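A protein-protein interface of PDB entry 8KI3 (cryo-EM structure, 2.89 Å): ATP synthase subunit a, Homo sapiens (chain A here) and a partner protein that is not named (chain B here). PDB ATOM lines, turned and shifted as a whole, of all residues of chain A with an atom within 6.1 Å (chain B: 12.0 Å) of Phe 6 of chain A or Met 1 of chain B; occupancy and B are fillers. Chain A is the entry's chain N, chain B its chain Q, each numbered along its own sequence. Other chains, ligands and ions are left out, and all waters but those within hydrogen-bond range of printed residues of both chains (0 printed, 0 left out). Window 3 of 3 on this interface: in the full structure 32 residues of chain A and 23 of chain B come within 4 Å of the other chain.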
ATOM      1  N   ASN A   4     -20.008  18.254 -10.065  1.00  0.00           N
ATOM      2  CA  ASN A   4     -20.982  17.529 -10.872  1.00  0.00           C
ATOM      3  C   ASN A   4     -20.470  16.149 -11.272  1.00  0.00           C
ATOM      4  O   ASN A   4     -21.251  15.222 -11.475  1.00  0.00           O
ATOM      5  CB  ASN A   4     -21.354  18.343 -12.114  1.00  0.00           C
ATOM      6  CG  ASN A   4     -20.149  18.695 -12.969  1.00  0.00           C
ATOM      7  OD1 ASN A   4     -19.027  18.278 -12.687  1.00  0.00           O
ATOM      8  ND2 ASN A   4     -20.382  19.467 -14.024  1.00  0.00           N
ATOM      9  N   LEU A   5     -19.151  16.023 -11.386  1.00  0.00           N
ATOM     10  CA  LEU A   5     -18.508  14.750 -11.685  1.00  0.00           C
ATOM     11  C   LEU A   5     -18.061  14.014 -10.432  1.00  0.00           C
ATOM     12  O   LEU A   5     -18.161  12.786 -10.368  1.00  0.00           O
ATOM     13  CB  LEU A   5     -17.302  14.970 -12.603  1.00  0.00           C
ATOM     14  CG  LEU A   5     -16.519  13.722 -13.009  1.00  0.00           C
ATOM     15  CD1 LEU A   5     -17.390  12.813 -13.850  1.00  0.00           C
ATOM     16  CD2 LEU A   5     -15.254  14.101 -13.755  1.00  0.00           C
ATOM     17  N   PHE A   6     -17.586  14.745  -9.429  1.00  0.00           N
ATOM     18  CA  PHE A   6     -17.149  14.158  -8.172  1.00  0.00           C
ATOM     19  C   PHE A   6     -18.305  14.123  -7.185  1.00  0.00           C
ATOM     20  O   PHE A   6     -18.093  14.170  -5.970  1.00  0.00           O
ATOM     21  CB  PHE A   6     -15.984  14.949  -7.583  1.00  0.00           C
ATOM     22  CG  PHE A   6     -14.713  14.840  -8.369  1.00  0.00           C
ATOM     23  CD1 PHE A   6     -14.575  15.485  -9.582  1.00  0.00           C
ATOM     24  CD2 PHE A   6     -13.650  14.102  -7.884  1.00  0.00           C
ATOM     25  CE1 PHE A   6     -13.406  15.386 -10.299  1.00  0.00           C
ATOM     26  CE2 PHE A   6     -12.479  14.001  -8.596  1.00  0.00           C
ATOM     27  CZ  PHE A   6     -12.357  14.644  -9.805  1.00  0.00           C
ATOM     28  N   ALA A   7     -19.532  14.064  -7.700  1.00  0.00           N
ATOM     29  CA  ALA A   7     -20.703  14.118  -6.834  1.00  0.00           C
ATOM     30  C   ALA A   7     -20.773  12.908  -5.915  1.00  0.00           C
ATOM     31  O   ALA A   7     -21.184  13.026  -4.757  1.00  0.00           O
ATOM     32  CB  ALA A   7     -21.971  14.226  -7.676  1.00  0.00           C
ATOM     33  N   SER A   8     -20.372  11.744  -6.403  1.00  0.00           N
ATOM     34  CA  SER A   8     -20.439  10.528  -5.597  1.00  0.00           C
ATOM     35  C   SER A   8     -19.393  10.473  -4.515  1.00  0.00           C
ATOM     36  O   SER A   8     -19.276   9.428  -3.871  1.00  0.00           O
ATOM     37  CB  SER A   8     -20.310   9.300  -6.496  1.00  0.00           C
ATOM     38  OG  SER A   8     -21.408   9.209  -7.386  1.00  0.00           O
ATOM     39  N   PHE A   9     -18.626  11.535  -4.280  1.00  0.00           N
ATOM     40  CA  PHE A   9     -17.623  11.552  -3.231  1.00  0.00           C
ATOM     41  C   PHE A   9     -17.874  12.611  -2.170  1.00  0.00           C
ATOM     42  O   PHE A   9     -17.127  12.663  -1.188  1.00  0.00           O
ATOM     43  CB  PHE A   9     -16.224  11.764  -3.829  1.00  0.00           C
ATOM     44  CG  PHE A   9     -15.909  10.837  -4.963  1.00  0.00           C
ATOM     45  CD1 PHE A   9     -15.420  11.325  -6.156  1.00  0.00           C
ATOM     46  CD2 PHE A   9     -16.106   9.477  -4.839  1.00  0.00           C
ATOM     47  CE1 PHE A   9     -15.137  10.476  -7.200  1.00  0.00           C
ATOM     48  CE2 PHE A   9     -15.821   8.626  -5.881  1.00  0.00           C
ATOM     49  CZ  PHE A   9     -15.337   9.128  -7.060  1.00  0.00           C
ATOM     50  N   ILE A  10     -18.888  13.449  -2.336  1.00  0.00           N
ATOM     51  CA  ILE A  10     -19.233  14.446  -1.332  1.00  0.00           C
ATOM     52  C   ILE A  10     -19.973  13.763  -0.195  1.00  0.00           C
ATOM     53  O   ILE A  10     -20.766  12.841  -0.420  1.00  0.00           O
ATOM     54  CB  ILE A  10     -20.076  15.572  -1.956  1.00  0.00           C
ATOM     55  CG1 ILE A  10     -19.468  16.008  -3.287  1.00  0.00           C
ATOM     56  CG2 ILE A  10     -20.165  16.756  -1.017  1.00  0.00           C
ATOM     57  CD1 ILE A  10     -20.188  17.162  -3.933  1.00  0.00           C
ATOM     58  N   THR A 165     -11.114   5.764  -5.776  1.00  0.00           N
ATOM     59  CA  THR A 165     -11.611   6.945  -6.471  1.00  0.00           C
ATOM     60  C   THR A 165     -11.508   6.768  -7.979  1.00  0.00           C
ATOM     61  O   THR A 165     -12.501   6.880  -8.703  1.00  0.00           O
ATOM     62  CB  THR A 165     -10.828   8.178  -6.028  1.00  0.00           C
ATOM     63  OG1 THR A 165     -10.735   8.198  -4.601  1.00  0.00           O
ATOM     64  CG2 THR A 165     -11.509   9.437  -6.501  1.00  0.00           C
ATOM     65  N   LEU A 169     -14.397   6.641 -10.733  1.00  0.00           N
ATOM     66  CA  LEU A 169     -14.453   7.651 -11.783  1.00  0.00           C
ATOM     67  C   LEU A 169     -14.466   7.014 -13.161  1.00  0.00           C
ATOM     68  O   LEU A 169     -15.190   7.466 -14.053  1.00  0.00           O
ATOM     69  CB  LEU A 169     -13.275   8.609 -11.658  1.00  0.00           C
ATOM     70  CG  LEU A 169     -13.588   9.923 -10.957  1.00  0.00           C
ATOM     71  CD1 LEU A 169     -12.314  10.682 -10.675  1.00  0.00           C
ATOM     72  CD2 LEU A 169     -14.517  10.742 -11.823  1.00  0.00           C
ATOM     73  N   MET B   1     -12.181  18.366  -6.340  1.00  0.00           N
ATOM     74  CA  MET B   1     -11.961  17.336  -5.334  1.00  0.00           C
ATOM     75  C   MET B   1     -12.722  17.652  -4.057  1.00  0.00           C
ATOM     76  O   MET B   1     -12.391  18.606  -3.355  1.00  0.00           O
ATOM     77  CB  MET B   1     -10.470  17.188  -5.030  1.00  0.00           C
ATOM     78  CG  MET B   1      -9.666  16.577  -6.157  1.00  0.00           C
ATOM     79  SD  MET B   1      -9.759  14.781  -6.185  1.00  0.00           S
ATOM     80  CE  MET B   1      -8.655  14.370  -4.838  1.00  0.00           C
ATOM     81  N   PRO B   2     -13.749  16.854  -3.758  1.00  0.00           N
ATOM     82  CA  PRO B   2     -14.489  17.029  -2.507  1.00  0.00           C
ATOM     83  C   PRO B   2     -13.865  16.319  -1.320  1.00  0.00           C
ATOM     84  O   PRO B   2     -14.335  16.514  -0.191  1.00  0.00           O
ATOM     85  CB  PRO B   2     -15.854  16.426  -2.844  1.00  0.00           C
ATOM     86  CG  PRO B   2     -15.529  15.342  -3.795  1.00  0.00           C
ATOM     87  CD  PRO B   2     -14.337  15.800  -4.596  1.00  0.00           C
ATOM     88  N   GLN B   3     -12.834  15.502  -1.538  1.00  0.00           N
ATOM     89  CA  GLN B   3     -12.112  14.905  -0.423  1.00  0.00           C
ATOM     90  C   GLN B   3     -11.389  15.949   0.408  1.00  0.00           C
ATOM     91  O   GLN B   3     -11.078  15.691   1.575  1.00  0.00           O
ATOM     92  CB  GLN B   3     -11.105  13.878  -0.933  1.00  0.00           C
ATOM     93  CG  GLN B   3     -11.693  12.520  -1.213  1.00  0.00           C
ATOM     94  CD  GLN B   3     -12.155  12.369  -2.642  1.00  0.00           C
ATOM     95  OE1 GLN B   3     -12.496  13.348  -3.301  1.00  0.00           O
ATOM     96  NE2 GLN B   3     -12.171  11.139  -3.131  1.00  0.00           N
ATOM     97  N   LEU B   4     -11.119  17.120  -0.162  1.00  0.00           N
ATOM     98  CA  LEU B   4     -10.339  18.150   0.506  1.00  0.00           C
ATOM     99  C   LEU B   4     -11.183  19.079   1.364  1.00  0.00           C
ATOM    100  O   LEU B   4     -10.621  19.913   2.080  1.00  0.00           O
ATOM    101  CB  LEU B   4      -9.565  18.979  -0.521  1.00  0.00           C
ATOM    102  CG  LEU B   4      -8.219  18.440  -1.012  1.00  0.00           C
ATOM    103  CD1 LEU B   4      -7.272  18.280   0.158  1.00  0.00           C
ATOM    104  CD2 LEU B   4      -8.356  17.138  -1.777  1.00  0.00           C
ATOM    105  N   ASN B   5     -12.508  18.959   1.319  1.00  0.00           N
ATOM    106  CA  ASN B   5     -13.360  19.809   2.138  1.00  0.00           C
ATOM    107  C   ASN B   5     -13.278  19.367   3.591  1.00  0.00           C
ATOM    108  O   ASN B   5     -14.098  18.568   4.051  1.00  0.00           O
ATOM    109  CB  ASN B   5     -14.805  19.766   1.647  1.00  0.00           C
ATOM    110  CG  ASN B   5     -15.696  20.742   2.385  1.00  0.00           C
ATOM    111  OD1 ASN B   5     -16.199  20.445   3.467  1.00  0.00           O
ATOM    112  ND2 ASN B   5     -15.894  21.919   1.804  1.00  0.00           N
ATOM    113  N   THR B   6     -12.303  19.893   4.321  1.00  0.00           N
ATOM    114  CA  THR B   6     -11.957  19.429   5.660  1.00  0.00           C
ATOM    115  C   THR B   6     -13.012  19.719   6.692  1.00  0.00           C
ATOM    116  O   THR B   6     -12.757  19.434   7.865  1.00  0.00           O
ATOM    117  CB  THR B   6     -10.635  20.056   6.097  1.00  0.00           C
ATOM    118  OG1 THR B   6     -10.780  21.478   6.145  1.00  0.00           O
ATOM    119  CG2 THR B   6      -9.534  19.704   5.118  1.00  0.00           C
ATOM    120  N   THR B   7     -14.174  20.272   6.352  1.00  0.00           N
ATOM    121  CA  THR B   7     -15.196  20.521   7.357  1.00  0.00           C
ATOM    122  C   THR B   7     -15.958  19.262   7.744  1.00  0.00           C
ATOM    123  O   THR B   7     -16.620  19.254   8.787  1.00  0.00           O
ATOM    124  CB  THR B   7     -16.181  21.583   6.864  1.00  0.00           C
ATOM    125  OG1 THR B   7     -16.736  21.175   5.607  1.00  0.00           O
ATOM    126  CG2 THR B   7     -15.478  22.918   6.689  1.00  0.00           C
ATOM    127  N   VAL B   8     -15.877  18.204   6.940  1.00  0.00           N
ATOM    128  CA  VAL B   8     -16.603  16.970   7.219  1.00  0.00           C
ATOM    129  C   VAL B   8     -15.619  15.834   7.455  1.00  0.00           C
ATOM    130  O   VAL B   8     -15.928  14.669   7.187  1.00  0.00           O
ATOM    131  CB  VAL B   8     -17.573  16.620   6.077  1.00  0.00           C
ATOM    132  CG1 VAL B   8     -18.702  17.633   6.009  1.00  0.00           C
ATOM    133  CG2 VAL B   8     -16.832  16.549   4.756  1.00  0.00           C
ATOM    134  N   TRP B   9     -14.431  16.156   7.948  1.00  0.00           N
ATOM    135  CA  TRP B   9     -13.487  15.099   8.278  1.00  0.00           C
ATOM    136  C   TRP B   9     -13.880  14.421   9.589  1.00  0.00           C
ATOM    137  O   TRP B   9     -13.969  13.188   9.621  1.00  0.00           O
ATOM    138  CB  TRP B   9     -12.052  15.632   8.337  1.00  0.00           C
ATOM    139  CG  TRP B   9     -11.415  15.761   6.990  1.00  0.00           C
ATOM    140  CD1 TRP B   9     -12.051  15.960   5.804  1.00  0.00           C
ATOM    141  CD2 TRP B   9     -10.018  15.688   6.687  1.00  0.00           C
ATOM    142  NE1 TRP B   9     -11.140  16.023   4.781  1.00  0.00           N
ATOM    143  CE2 TRP B   9      -9.883  15.858   5.298  1.00  0.00           C
ATOM    144  CE3 TRP B   9      -8.869  15.497   7.455  1.00  0.00           C
ATOM    145  CZ2 TRP B   9      -8.648  15.843   4.662  1.00  0.00           C
ATOM    146  CZ3 TRP B   9      -7.643  15.483   6.820  1.00  0.00           C
ATOM    147  CH2 TRP B   9      -7.543  15.655   5.439  1.00  0.00           C
ATOM    148  N   MET B  12     -16.070  11.525   9.307  1.00  0.00           N
ATOM    149  CA  MET B  12     -15.546  10.275   8.778  1.00  0.00           C
ATOM    150  C   MET B  12     -14.551   9.598   9.705  1.00  0.00           C
ATOM    151  O   MET B  12     -14.360   8.383   9.597  1.00  0.00           O
ATOM    152  CB  MET B  12     -14.867  10.506   7.424  1.00  0.00           C
ATOM    153  CG  MET B  12     -15.697  11.275   6.424  1.00  0.00           C
ATOM    154  SD  MET B  12     -17.084  10.337   5.770  1.00  0.00           S
ATOM    155  CE  MET B  12     -17.923  11.619   4.851  1.00  0.00           C
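Hydrophobic or aromatic side chains of chain B that line the printed part of chain A: Met 1 and Pro 2.
Among the printed residues, 5 pairs touch across the chains.
Among the printed residues, no Asp or Glu carboxylate lies within 4 Å of a Lys or Arg side-chain nitrogen of the other chain.
CE2 of Phe 6 of chain A touches SD of Met 1 of chain B (3.7 Å).
Pro 2 of chain B touches Phe 6 of chain A.
CG of Pro 2 of chain B touches CB of Phe 9 of chain A (3.6 Å).
Ile 10 of chain A touches Pro 2 of chain B.
Thr 165 of chain A touches Gln 3 of chain B (OG1 to NE2, 3.6 Å).
No residue of chain B comes within 4 Å of Asn 4 of chain A.
No residue of chain B comes within 4 Å of Leu 5 of chain A.
Printed residues of chain B within 4 Å of Phe 6 of chain A: Met 1 and Pro 2.
Ala 7 of chain A touches none of the printed residues of chain B.
Ser 8 of chain A touches none of the printed residues of chain B.
Of chain B, only Pro 2 (3.6 Å) comes within 4 Å of Phe 9 of chain A.
Ile 10 of chain A touches one residue of chain B.
Printed residues of chain A within 4 Å of Pro 2 of chain B: Phe 6, Phe 9 and Ile 10.
Of the printed residues of chain A, Gln 3 of chain B touches Thr 165.
Thr 7 of chain B touches none of the printed residues of chain A.
The backbone carbonyl oxygen (O) of Gln 3 of chain B lies within hydrogen-bond range of the indole nitrogen (NE1) of Trp 9 of chain B (3.2 Å).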
